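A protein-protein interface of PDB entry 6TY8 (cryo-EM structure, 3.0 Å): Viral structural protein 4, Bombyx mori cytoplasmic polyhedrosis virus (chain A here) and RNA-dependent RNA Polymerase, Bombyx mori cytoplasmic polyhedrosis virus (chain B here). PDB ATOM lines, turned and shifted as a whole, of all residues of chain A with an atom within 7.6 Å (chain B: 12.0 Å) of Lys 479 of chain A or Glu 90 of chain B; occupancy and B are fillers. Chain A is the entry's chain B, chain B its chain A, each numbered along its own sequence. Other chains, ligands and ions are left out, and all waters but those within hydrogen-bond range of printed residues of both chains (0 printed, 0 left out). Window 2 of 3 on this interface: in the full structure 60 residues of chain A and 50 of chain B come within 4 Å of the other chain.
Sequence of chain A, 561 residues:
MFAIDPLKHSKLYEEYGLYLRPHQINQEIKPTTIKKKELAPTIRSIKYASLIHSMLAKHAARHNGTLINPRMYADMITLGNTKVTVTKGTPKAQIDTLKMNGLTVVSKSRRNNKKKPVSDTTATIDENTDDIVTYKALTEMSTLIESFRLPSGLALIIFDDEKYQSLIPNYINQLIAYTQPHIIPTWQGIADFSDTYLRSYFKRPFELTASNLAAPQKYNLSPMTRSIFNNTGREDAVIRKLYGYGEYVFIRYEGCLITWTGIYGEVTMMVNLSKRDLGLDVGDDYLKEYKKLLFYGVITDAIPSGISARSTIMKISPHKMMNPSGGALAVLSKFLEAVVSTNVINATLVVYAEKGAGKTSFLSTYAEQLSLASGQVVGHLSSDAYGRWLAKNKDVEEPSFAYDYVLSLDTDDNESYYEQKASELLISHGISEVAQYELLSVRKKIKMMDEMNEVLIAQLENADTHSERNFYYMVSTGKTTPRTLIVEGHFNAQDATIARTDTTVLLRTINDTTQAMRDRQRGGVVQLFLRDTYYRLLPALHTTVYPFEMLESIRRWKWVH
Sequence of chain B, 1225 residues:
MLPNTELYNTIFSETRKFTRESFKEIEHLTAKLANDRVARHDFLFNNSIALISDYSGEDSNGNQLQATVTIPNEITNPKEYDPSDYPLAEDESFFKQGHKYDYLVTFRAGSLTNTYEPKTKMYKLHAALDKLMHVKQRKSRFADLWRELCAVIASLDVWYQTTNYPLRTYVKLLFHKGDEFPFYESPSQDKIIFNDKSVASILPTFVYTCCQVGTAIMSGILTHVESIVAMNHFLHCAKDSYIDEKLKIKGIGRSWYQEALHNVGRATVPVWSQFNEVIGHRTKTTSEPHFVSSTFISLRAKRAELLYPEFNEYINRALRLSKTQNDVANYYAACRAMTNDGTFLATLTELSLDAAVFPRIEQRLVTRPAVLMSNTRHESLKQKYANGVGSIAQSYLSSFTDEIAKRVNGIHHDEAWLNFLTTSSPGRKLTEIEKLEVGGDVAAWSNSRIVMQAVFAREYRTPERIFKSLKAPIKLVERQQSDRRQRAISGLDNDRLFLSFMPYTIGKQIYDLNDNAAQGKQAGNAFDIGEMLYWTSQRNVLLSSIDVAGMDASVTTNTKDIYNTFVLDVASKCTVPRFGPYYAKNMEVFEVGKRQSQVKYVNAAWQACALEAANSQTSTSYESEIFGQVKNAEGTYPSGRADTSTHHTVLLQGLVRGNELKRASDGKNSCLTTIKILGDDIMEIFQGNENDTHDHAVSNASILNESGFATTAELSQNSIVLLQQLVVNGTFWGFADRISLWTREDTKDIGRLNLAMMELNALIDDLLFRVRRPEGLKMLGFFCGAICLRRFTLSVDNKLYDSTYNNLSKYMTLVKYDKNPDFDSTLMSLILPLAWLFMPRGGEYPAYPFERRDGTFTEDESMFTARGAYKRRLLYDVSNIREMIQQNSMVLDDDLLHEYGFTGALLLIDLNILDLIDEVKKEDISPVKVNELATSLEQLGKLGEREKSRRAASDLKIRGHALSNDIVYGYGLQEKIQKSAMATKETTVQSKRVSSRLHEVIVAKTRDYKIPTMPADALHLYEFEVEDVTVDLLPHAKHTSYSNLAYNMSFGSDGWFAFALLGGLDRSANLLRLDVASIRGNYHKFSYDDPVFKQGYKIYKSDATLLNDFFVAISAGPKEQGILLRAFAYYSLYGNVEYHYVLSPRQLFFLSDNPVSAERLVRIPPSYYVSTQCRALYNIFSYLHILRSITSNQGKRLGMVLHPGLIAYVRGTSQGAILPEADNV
O of Thr 477 of chain A is in hydrogen-bond range of N of Asp 91 of chain B.
The backbone NH of Gln 97 of chain B sits at hydrogen-bond distance from the side-chain hydroxyl of Tyr 473 of chain A (3.2 Å).
The backbone carbonyl oxygen (O) of Phe 94 of chain B sits at hydrogen-bond distance from the backbone NH (N) of Ala 89 of chain B (2.9 Å).
The backbone carbonyl oxygen of Tyr 473 of chain A is in hydrogen-bond range of the side-chain hydroxyl of Thr 477 of chain A, 2.7 Å away.
O of Lys 96 of chain B lies within hydrogen-bond range of ND1 of His 99 of chain B (2.7 Å).
The backbone carbonyl oxygen (O) of Pro 87 of chain B is in hydrogen-bond range of the backbone NH (N) of Lys 96 of chain B (3.2 Å).
Among the printed residues, merely in contact across the chains: Lys 479 of chain A with Glu 90 of chain B (3.2 Å), Tyr 473 of chain A with Lys 96 of chain B (3.5 Å), Thr 477 of chain A with Glu 90 of chain B (3.5 Å), Tyr 473 of chain A with Ala 89 of chain B (3.6 Å), Tyr 473 of chain A with Phe 95 of chain B (3.7 Å), Gly 478 of chain A with Asp 91 of chain B (3.8 Å), Met 474 of chain A with Glu 90 of chain B (3.9 Å) and Thr 477 of chain A with Ala 89 of chain B (3.96 Å).
Printed residues of chain B within 4 Å of Lys 479 of chain A: Glu 90 (3.2 Å).
Of the printed residues of chain A, Glu 90 of chain B touches Met 474, Thr 477 and Lys 479.
Of the printed residues of chain B, Thr 477 of chain A touches Ala 89 (3.96 Å), Glu 90 (3.5 Å) and Asp 91 (3.2 Å).
Thr 481 of chain A touches none of the printed residues of chain B.
Printed residues of chain A within 4 Å of Gln 97 of chain B: Tyr 473 (3.2 Å).
Of the printed residues of chain B, Tyr 473 of chain A touches Ala 89, Phe 95, Lys 96 and Gln 97.
Of the printed residues of chain A, Lys 96 of chain B touches Tyr 473.
Of the printed residues of chain A, Asp 91 of chain B touches Thr 477 and Gly 478.
Printed residues of chain A within 4 Å of Phe 95 of chain B: Tyr 473.
The nearest residue of chain B that does not touch Lys 479 of chain A is Asp 91 of chain B (5.0 Å).
Of the 18 printed residues of chain B, 6 touch a printed residue of chain A.
Printed residues of chain B that touch a printed residue of chain A: Ala 89, Glu 90, Asp 91, Phe 95, Lys 96 and Gln 97.
Hydrophobic or aromatic side chains of chain B within 4 Å of the printed part of chain A: Ala 89.
Among the printed residues, 10 pairs touch across the chains.
Among the printed residues, no Asp or Glu carboxylate lies within 4 Å of a Lys or Arg side-chain nitrogen of the other chain.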
ATOM      1  N   PHE A 401     -10.201  -7.852   5.982  1.00  0.00           N
ATOM      2  CA  PHE A 401     -10.624  -7.412   4.661  1.00  0.00           C
ATOM      3  C   PHE A 401     -11.524  -6.187   4.716  1.00  0.00           C
ATOM      4  O   PHE A 401     -12.338  -5.995   3.808  1.00  0.00           O
ATOM      5  CB  PHE A 401     -11.354  -8.540   3.936  1.00  0.00           C
ATOM      6  CG  PHE A 401     -10.478  -9.694   3.560  1.00  0.00           C
ATOM      7  CD1 PHE A 401      -9.704  -9.649   2.417  1.00  0.00           C
ATOM      8  CD2 PHE A 401     -10.451 -10.835   4.335  1.00  0.00           C
ATOM      9  CE1 PHE A 401      -8.911 -10.714   2.064  1.00  0.00           C
ATOM     10  CE2 PHE A 401      -9.657 -11.899   3.991  1.00  0.00           C
ATOM     11  CZ  PHE A 401      -8.886 -11.840   2.855  1.00  0.00           C
ATOM     12  N   TYR A 473     -12.872 -10.519  -3.780  1.00  0.00           N
ATOM     13  CA  TYR A 473     -14.150 -11.073  -3.345  1.00  0.00           C
ATOM     14  C   TYR A 473     -14.566 -10.561  -1.975  1.00  0.00           C
ATOM     15  O   TYR A 473     -15.706 -10.119  -1.801  1.00  0.00           O
ATOM     16  CB  TYR A 473     -14.074 -12.598  -3.329  1.00  0.00           C
ATOM     17  CG  TYR A 473     -15.270 -13.269  -2.706  1.00  0.00           C
ATOM     18  CD1 TYR A 473     -16.495 -13.289  -3.347  1.00  0.00           C
ATOM     19  CD2 TYR A 473     -15.162 -13.908  -1.480  1.00  0.00           C
ATOM     20  CE1 TYR A 473     -17.587 -13.907  -2.776  1.00  0.00           C
ATOM     21  CE2 TYR A 473     -16.246 -14.527  -0.903  1.00  0.00           C
ATOM     22  CZ  TYR A 473     -17.450 -14.527  -1.556  1.00  0.00           C
ATOM     23  OH  TYR A 473     -18.528 -15.146  -0.977  1.00  0.00           O
ATOM     24  N   MET A 474     -13.670 -10.621  -0.993  1.00  0.00           N
ATOM     25  CA  MET A 474     -14.017 -10.183   0.350  1.00  0.00           C
ATOM     26  C   MET A 474     -14.100  -8.669   0.471  1.00  0.00           C
ATOM     27  O   MET A 474     -14.705  -8.175   1.425  1.00  0.00           O
ATOM     28  CB  MET A 474     -13.008 -10.730   1.354  1.00  0.00           C
ATOM     29  CG  MET A 474     -13.014 -12.241   1.472  1.00  0.00           C
ATOM     30  SD  MET A 474     -14.573 -12.891   2.080  1.00  0.00           S
ATOM     31  CE  MET A 474     -14.522 -12.337   3.779  1.00  0.00           C
ATOM     32  N   VAL A 475     -13.504  -7.923  -0.458  1.00  0.00           N
ATOM     33  CA  VAL A 475     -13.710  -6.479  -0.452  1.00  0.00           C
ATOM     34  C   VAL A 475     -15.009  -6.117  -1.172  1.00  0.00           C
ATOM     35  O   VAL A 475     -15.737  -5.217  -0.740  1.00  0.00           O
ATOM     36  CB  VAL A 475     -12.475  -5.772  -1.047  1.00  0.00           C
ATOM     37  CG1 VAL A 475     -12.707  -4.295  -1.236  1.00  0.00           C
ATOM     38  CG2 VAL A 475     -11.296  -5.938  -0.123  1.00  0.00           C
ATOM     39  N   SER A 476     -15.365  -6.848  -2.234  1.00  0.00           N
ATOM     40  CA  SER A 476     -16.591  -6.534  -2.965  1.00  0.00           C
ATOM     41  C   SER A 476     -17.841  -6.959  -2.210  1.00  0.00           C
ATOM     42  O   SER A 476     -18.851  -6.250  -2.244  1.00  0.00           O
ATOM     43  CB  SER A 476     -16.572  -7.198  -4.339  1.00  0.00           C
ATOM     44  OG  SER A 476     -15.521  -6.698  -5.141  1.00  0.00           O
ATOM     45  N   THR A 477     -17.804  -8.103  -1.532  1.00  0.00           N
ATOM     46  CA  THR A 477     -18.978  -8.649  -0.870  1.00  0.00           C
ATOM     47  C   THR A 477     -18.989  -8.385   0.629  1.00  0.00           C
ATOM     48  O   THR A 477     -19.393  -9.260   1.397  1.00  0.00           O
ATOM     49  CB  THR A 477     -19.072 -10.148  -1.126  1.00  0.00           C
ATOM     50  OG1 THR A 477     -17.973 -10.805  -0.493  1.00  0.00           O
ATOM     51  CG2 THR A 477     -19.008 -10.421  -2.605  1.00  0.00           C
ATOM     52  N   GLY A 478     -18.544  -7.217   1.063  1.00  0.00           N
ATOM     53  CA  GLY A 478     -18.484  -6.925   2.479  1.00  0.00           C
ATOM     54  C   GLY A 478     -19.710  -6.184   2.980  1.00  0.00           C
ATOM     55  O   GLY A 478     -20.537  -5.671   2.229  1.00  0.00           O
ATOM     56  N   LYS A 479     -19.816  -6.137   4.309  1.00  0.00           N
ATOM     57  CA  LYS A 479     -20.894  -5.403   4.964  1.00  0.00           C
ATOM     58  C   LYS A 479     -20.736  -3.901   4.778  1.00  0.00           C
ATOM     59  O   LYS A 479     -21.644  -3.224   4.283  1.00  0.00           O
ATOM     60  CB  LYS A 479     -20.910  -5.733   6.456  1.00  0.00           C
ATOM     61  CG  LYS A 479     -21.251  -7.155   6.832  1.00  0.00           C
ATOM     62  CD  LYS A 479     -22.738  -7.417   6.732  1.00  0.00           C
ATOM     63  CE  LYS A 479     -23.069  -8.803   7.259  1.00  0.00           C
ATOM     64  NZ  LYS A 479     -22.807  -8.913   8.718  1.00  0.00           N
ATOM     65  N   THR A 480     -19.593  -3.361   5.187  1.00  0.00           N
ATOM     66  CA  THR A 480     -19.370  -1.925   5.246  1.00  0.00           C
ATOM     67  C   THR A 480     -18.827  -1.348   3.948  1.00  0.00           C
ATOM     68  O   THR A 480     -18.598  -0.136   3.878  1.00  0.00           O
ATOM     69  CB  THR A 480     -18.401  -1.595   6.383  1.00  0.00           C
ATOM     70  OG1 THR A 480     -17.134  -2.205   6.118  1.00  0.00           O
ATOM     71  CG2 THR A 480     -18.935  -2.116   7.705  1.00  0.00           C
ATOM     72  N   THR A 481     -18.611  -2.171   2.936  1.00  0.00           N
ATOM     73  CA  THR A 481     -18.029  -1.683   1.701  1.00  0.00           C
ATOM     74  C   THR A 481     -19.080  -0.922   0.889  1.00  0.00           C
ATOM     75  O   THR A 481     -20.282  -1.148   1.051  1.00  0.00           O
ATOM     76  CB  THR A 481     -17.450  -2.850   0.896  1.00  0.00           C
ATOM     77  OG1 THR A 481     -16.694  -2.360  -0.215  1.00  0.00           O
ATOM     78  CG2 THR A 481     -18.530  -3.775   0.388  1.00  0.00           C
ATOM     79  N   PRO A 482     -18.660   0.054   0.082  1.00  0.00           N
ATOM     80  CA  PRO A 482     -19.618   0.763  -0.767  1.00  0.00           C
ATOM     81  C   PRO A 482     -20.198  -0.130  -1.850  1.00  0.00           C
ATOM     82  O   PRO A 482     -19.619  -1.141  -2.249  1.00  0.00           O
ATOM     83  CB  PRO A 482     -18.786   1.900  -1.364  1.00  0.00           C
ATOM     84  CG  PRO A 482     -17.739   2.137  -0.358  1.00  0.00           C
ATOM     85  CD  PRO A 482     -17.393   0.795   0.188  1.00  0.00           C
ATOM     86  N   ARG A 483     -21.393   0.253  -2.298  1.00  0.00           N
ATOM     87  CA  ARG A 483     -22.094  -0.500  -3.330  1.00  0.00           C
ATOM     88  C   ARG A 483     -21.372  -0.413  -4.666  1.00  0.00           C
ATOM     89  O   ARG A 483     -20.950  -1.431  -5.223  1.00  0.00           O
ATOM     90  CB  ARG A 483     -23.518   0.032  -3.460  1.00  0.00           C
ATOM     91  CG  ARG A 483     -24.333  -0.638  -4.525  1.00  0.00           C
ATOM     92  CD  ARG A 483     -25.724  -0.042  -4.583  1.00  0.00           C
ATOM     93  NE  ARG A 483     -26.560  -0.747  -5.544  1.00  0.00           N
ATOM     94  CZ  ARG A 483     -26.675  -0.411  -6.820  1.00  0.00           C
ATOM     95  NH1 ARG A 483     -26.021   0.633  -7.292  1.00  0.00           N
ATOM     96  NH2 ARG A 483     -27.457  -1.114  -7.618  1.00  0.00           N
ATOM     97  N   TYR B  86     -25.979 -24.197   2.675  1.00  0.00           N
ATOM     98  CA  TYR B  86     -26.053 -23.247   1.570  1.00  0.00           C
ATOM     99  C   TYR B  86     -25.780 -21.846   2.108  1.00  0.00           C
ATOM    100  O   TYR B  86     -26.709 -21.056   2.310  1.00  0.00           O
ATOM    101  CB  TYR B  86     -27.415 -23.325   0.889  1.00  0.00           C
ATOM    102  CG  TYR B  86     -27.676 -24.680   0.286  1.00  0.00           C
ATOM    103  CD1 TYR B  86     -27.145 -25.024  -0.948  1.00  0.00           C
ATOM    104  CD2 TYR B  86     -28.435 -25.625   0.962  1.00  0.00           C
ATOM    105  CE1 TYR B  86     -27.375 -26.268  -1.495  1.00  0.00           C
ATOM    106  CE2 TYR B  86     -28.670 -26.872   0.419  1.00  0.00           C
ATOM    107  CZ  TYR B  86     -28.136 -27.185  -0.807  1.00  0.00           C
ATOM    108  OH  TYR B  86     -28.366 -28.422  -1.350  1.00  0.00           O
ATOM    109  N   PRO B  87     -24.519 -21.510   2.357  1.00  0.00           N
ATOM    110  CA  PRO B  87     -24.210 -20.214   2.954  1.00  0.00           C
ATOM    111  C   PRO B  87     -24.209 -19.123   1.899  1.00  0.00           C
ATOM    112  O   PRO B  87     -24.138 -19.377   0.697  1.00  0.00           O
ATOM    113  CB  PRO B  87     -22.811 -20.421   3.527  1.00  0.00           C
ATOM    114  CG  PRO B  87     -22.197 -21.375   2.585  1.00  0.00           C
ATOM    115  CD  PRO B  87     -23.293 -22.291   2.119  1.00  0.00           C
ATOM    116  N   LEU B  88     -24.288 -17.890   2.374  1.00  0.00           N
ATOM    117  CA  LEU B  88     -24.268 -16.726   1.511  1.00  0.00           C
ATOM    118  C   LEU B  88     -23.023 -15.897   1.777  1.00  0.00           C
ATOM    119  O   LEU B  88     -22.258 -16.152   2.708  1.00  0.00           O
ATOM    120  CB  LEU B  88     -25.527 -15.884   1.722  1.00  0.00           C
ATOM    121  CG  LEU B  88     -26.794 -16.574   1.247  1.00  0.00           C
ATOM    122  CD1 LEU B  88     -28.007 -15.753   1.609  1.00  0.00           C
ATOM    123  CD2 LEU B  88     -26.709 -16.765  -0.238  1.00  0.00           C
ATOM    124  N   ALA B  89     -22.826 -14.891   0.938  1.00  0.00           N
ATOM    125  CA  ALA B  89     -21.787 -13.920   1.213  1.00  0.00           C
ATOM    126  C   ALA B  89     -22.256 -12.970   2.307  1.00  0.00           C
ATOM    127  O   ALA B  89     -23.427 -12.963   2.698  1.00  0.00           O
ATOM    128  CB  ALA B  89     -21.423 -13.151  -0.053  1.00  0.00           C
ATOM    129  N   GLU B  90     -21.320 -12.165   2.813  1.00  0.00           N
ATOM    130  CA  GLU B  90     -21.645 -11.235   3.890  1.00  0.00           C
ATOM    131  C   GLU B  90     -22.578 -10.135   3.405  1.00  0.00           C
ATOM    132  O   GLU B  90     -23.439  -9.661   4.147  1.00  0.00           O
ATOM    133  CB  GLU B  90     -20.363 -10.648   4.478  1.00  0.00           C
ATOM    134  CG  GLU B  90     -19.569 -11.625   5.327  1.00  0.00           C
ATOM    135  CD  GLU B  90     -18.677 -12.543   4.516  1.00  0.00           C
ATOM    136  OE1 GLU B  90     -18.610 -12.387   3.277  1.00  0.00           O
ATOM    137  OE2 GLU B  90     -18.046 -13.433   5.120  1.00  0.00           O
ATOM    138  N   ASP B  91     -22.446  -9.741   2.141  1.00  0.00           N
ATOM    139  CA  ASP B  91     -23.398  -8.809   1.563  1.00  0.00           C
ATOM    140  C   ASP B  91     -24.705  -9.495   1.190  1.00  0.00           C
ATOM    141  O   ASP B  91     -25.698  -8.800   0.939  1.00  0.00           O
ATOM    142  CB  ASP B  91     -22.774  -8.143   0.333  1.00  0.00           C
ATOM    143  CG  ASP B  91     -23.415  -6.809  -0.016  1.00  0.00           C
ATOM    144  OD1 ASP B  91     -24.319  -6.355   0.715  1.00  0.00           O
ATOM    145  OD2 ASP B  91     -23.002  -6.201  -1.026  1.00  0.00           O
ATOM    146  N   GLU B  92     -24.723 -10.838   1.186  1.00  0.00           N
ATOM    147  CA  GLU B  92     -25.819 -11.665   0.672  1.00  0.00           C
ATOM    148  C   GLU B  92     -26.176 -11.283  -0.759  1.00  0.00           C
ATOM    149  O   GLU B  92     -27.346 -11.162  -1.121  1.00  0.00           O
ATOM    150  CB  GLU B  92     -27.045 -11.620   1.583  1.00  0.00           C
ATOM    151  CG  GLU B  92     -26.824 -12.299   2.915  1.00  0.00           C
ATOM    152  CD  GLU B  92     -28.026 -12.208   3.833  1.00  0.00           C
ATOM    153  OE1 GLU B  92     -28.995 -11.506   3.482  1.00  0.00           O
ATOM    154  OE2 GLU B  92     -27.999 -12.840   4.909  1.00  0.00           O
ATOM    155  N   SER B  93     -25.151 -11.084  -1.576  1.00  0.00           N
ATOM    156  CA  SER B  93     -25.332 -10.787  -2.984  1.00  0.00           C
ATOM    157  C   SER B  93     -25.244 -12.025  -3.859  1.00  0.00           C
ATOM    158  O   SER B  93     -25.686 -11.978  -5.011  1.00  0.00           O
ATOM    159  CB  SER B  93     -24.303  -9.748  -3.437  1.00  0.00           C
ATOM    160  OG  SER B  93     -22.983 -10.232  -3.291  1.00  0.00           O
ATOM    161  N   PHE B  94     -24.702 -13.124  -3.334  1.00  0.00           N
ATOM    162  CA  PHE B  94     -24.561 -14.405  -4.017  1.00  0.00           C
ATOM    163  C   PHE B  94     -24.147 -15.402  -2.938  1.00  0.00           C
ATOM    164  O   PHE B  94     -23.887 -15.021  -1.794  1.00  0.00           O
ATOM    165  CB  PHE B  94     -23.535 -14.329  -5.156  1.00  0.00           C
ATOM    166  CG  PHE B  94     -23.614 -15.464  -6.131  1.00  0.00           C
ATOM    167  CD1 PHE B  94     -24.692 -15.576  -6.982  1.00  0.00           C
ATOM    168  CD2 PHE B  94     -22.590 -16.386  -6.232  1.00  0.00           C
ATOM    169  CE1 PHE B  94     -24.769 -16.606  -7.887  1.00  0.00           C
ATOM    170  CE2 PHE B  94     -22.662 -17.416  -7.138  1.00  0.00           C
ATOM    171  CZ  PHE B  94     -23.748 -17.521  -7.969  1.00  0.00           C
ATOM    172  N   PHE B  95     -24.089 -16.681  -3.310  1.00  0.00           N
ATOM    173  CA  PHE B  95     -23.614 -17.716  -2.400  1.00  0.00           C
ATOM    174  C   PHE B  95     -22.139 -17.520  -2.068  1.00  0.00           C
ATOM    175  O   PHE B  95     -21.427 -16.749  -2.716  1.00  0.00           O
ATOM    176  CB  PHE B  95     -23.813 -19.104  -3.012  1.00  0.00           C
ATOM    177  CG  PHE B  95     -25.250 -19.507  -3.163  1.00  0.00           C
ATOM    178  CD1 PHE B  95     -25.973 -19.969  -2.077  1.00  0.00           C
ATOM    179  CD2 PHE B  95     -25.871 -19.446  -4.398  1.00  0.00           C
ATOM    180  CE1 PHE B  95     -27.292 -20.344  -2.216  1.00  0.00           C
ATOM    181  CE2 PHE B  95     -27.187 -19.821  -4.543  1.00  0.00           C
ATOM    182  CZ  PHE B  95     -27.900 -20.266  -3.451  1.00  0.00           C
ATOM    183  N   LYS B  96     -21.685 -18.233  -1.041  1.00  0.00           N
ATOM    184  CA  LYS B  96     -20.295 -18.155  -0.616  1.00  0.00           C
ATOM    185  C   LYS B  96     -19.392 -18.736  -1.698  1.00  0.00           C
ATOM    186  O   LYS B  96     -19.811 -19.594  -2.479  1.00  0.00           O
ATOM    187  CB  LYS B  96     -20.122 -18.908   0.705  1.00  0.00           C
ATOM    188  CG  LYS B  96     -18.786 -18.754   1.399  1.00  0.00           C
ATOM    189  CD  LYS B  96     -18.747 -19.559   2.671  1.00  0.00           C
ATOM    190  CE  LYS B  96     -17.444 -19.347   3.398  1.00  0.00           C
ATOM    191  NZ  LYS B  96     -16.306 -19.919   2.632  1.00  0.00           N
ATOM    192  N   GLN B  97     -18.161 -18.217  -1.770  1.00  0.00           N
ATOM    193  CA  GLN B  97     -17.192 -18.549  -2.809  1.00  0.00           C
ATOM    194  C   GLN B  97     -16.871 -20.033  -2.865  1.00  0.00           C
ATOM    195  O   GLN B  97     -17.162 -20.699  -3.862  1.00  0.00           O
ATOM    196  CB  GLN B  97     -15.899 -17.771  -2.585  1.00  0.00           C
ATOM    197  CG  GLN B  97     -14.870 -17.978  -3.673  1.00  0.00           C
ATOM    198  CD  GLN B  97     -13.589 -17.234  -3.405  1.00  0.00           C
ATOM    199  OE1 GLN B  97     -13.425 -16.608  -2.362  1.00  0.00           O
ATOM    200  NE2 GLN B  97     -12.668 -17.294  -4.351  1.00  0.00           N
ATOM    201  N   GLY B  98     -16.268 -20.563  -1.807  1.00  0.00           N
ATOM    202  CA  GLY B  98     -16.065 -21.992  -1.713  1.00  0.00           C
ATOM    203  C   GLY B  98     -17.170 -22.627  -0.901  1.00  0.00           C
ATOM    204  O   GLY B  98     -17.115 -22.624   0.339  1.00  0.00           O
ATOM    205  N   HIS B  99     -18.180 -23.169  -1.571  1.00  0.00           N
ATOM    206  CA  HIS B  99     -19.225 -23.912  -0.886  1.00  0.00           C
ATOM    207  C   HIS B  99     -19.265 -25.314  -1.466  1.00  0.00           C
ATOM    208  O   HIS B  99     -19.156 -25.496  -2.680  1.00  0.00           O
ATOM    209  CB  HIS B  99     -20.587 -23.220  -0.995  1.00  0.00           C
ATOM    210  CG  HIS B  99     -21.078 -23.050  -2.395  1.00  0.00           C
ATOM    211  ND1 HIS B  99     -20.658 -22.024  -3.209  1.00  0.00           N
ATOM    212  CD2 HIS B  99     -21.970 -23.764  -3.121  1.00  0.00           C
ATOM    213  CE1 HIS B  99     -21.261 -22.117  -4.380  1.00  0.00           C
ATOM    214  NE2 HIS B  99     -22.063 -23.165  -4.352  1.00  0.00           N
ATOM    215  N   LYS B 121     -34.582 -11.818   1.620  1.00  0.00           N
ATOM    216  CA  LYS B 121     -33.518 -12.587   0.981  1.00  0.00           C
ATOM    217  C   LYS B 121     -33.625 -14.065   1.331  1.00  0.00           C
ATOM    218  O   LYS B 121     -33.554 -14.935   0.451  1.00  0.00           O
ATOM    219  CB  LYS B 121     -32.150 -12.043   1.389  1.00  0.00           C
ATOM    220  CG  LYS B 121     -31.872 -10.644   0.900  1.00  0.00           C
ATOM    221  CD  LYS B 121     -31.828 -10.628  -0.608  1.00  0.00           C
ATOM    222  CE  LYS B 121     -30.620 -11.381  -1.113  1.00  0.00           C
ATOM    223  NZ  LYS B 121     -30.527 -11.307  -2.591  1.00  0.00           N
ATOM    224  N   MET B 122     -33.809 -14.363   2.616  1.00  0.00           N
ATOM    225  CA  MET B 122     -33.886 -15.747   3.055  1.00  0.00           C
ATOM    226  C   MET B 122     -35.168 -16.414   2.590  1.00  0.00           C
ATOM    227  O   MET B 122     -35.170 -17.619   2.341  1.00  0.00           O
ATOM    228  CB  MET B 122     -33.766 -15.821   4.572  1.00  0.00           C
ATOM    229  CG  MET B 122     -32.424 -15.347   5.089  1.00  0.00           C
ATOM    230  SD  MET B 122     -31.048 -16.319   4.460  1.00  0.00           S
ATOM    231  CE  MET B 122     -31.316 -17.860   5.323  1.00  0.00           C
ATOM    232  N   LEU B 125     -34.449 -17.422  -0.949  1.00  0.00           N
ATOM    233  CA  LEU B 125     -33.541 -18.568  -0.967  1.00  0.00           C
ATOM    234  C   LEU B 125     -34.259 -19.855  -0.575  1.00  0.00           C
ATOM    235  O   LEU B 125     -34.057 -20.901  -1.199  1.00  0.00           O
ATOM    236  CB  LEU B 125     -32.344 -18.305  -0.059  1.00  0.00           C
ATOM    237  CG  LEU B 125     -31.206 -19.321  -0.054  1.00  0.00           C
ATOM    238  CD1 LEU B 125     -29.924 -18.579   0.024  1.00  0.00           C
ATOM    239  CD2 LEU B 125     -31.284 -20.212   1.158  1.00  0.00           C
ATOM    240  N   PHE B 627     -31.242 -13.195  -6.242  1.00  0.00           N
ATOM    241  CA  PHE B 627     -30.256 -12.128  -6.168  1.00  0.00           C
ATOM    242  C   PHE B 627     -30.424 -11.062  -7.242  1.00  0.00           C
ATOM    243  O   PHE B 627     -29.664 -10.090  -7.246  1.00  0.00           O
ATOM    244  CB  PHE B 627     -28.854 -12.715  -6.276  1.00  0.00           C
ATOM    245  CG  PHE B 627     -28.567 -13.788  -5.277  1.00  0.00           C
ATOM    246  CD1 PHE B 627     -28.335 -13.483  -3.953  1.00  0.00           C
ATOM    247  CD2 PHE B 627     -28.488 -15.107  -5.679  1.00  0.00           C
ATOM    248  CE1 PHE B 627     -28.060 -14.480  -3.041  1.00  0.00           C
ATOM    249  CE2 PHE B 627     -28.208 -16.101  -4.776  1.00  0.00           C
ATOM    250  CZ  PHE B 627     -27.992 -15.788  -3.457  1.00  0.00           C
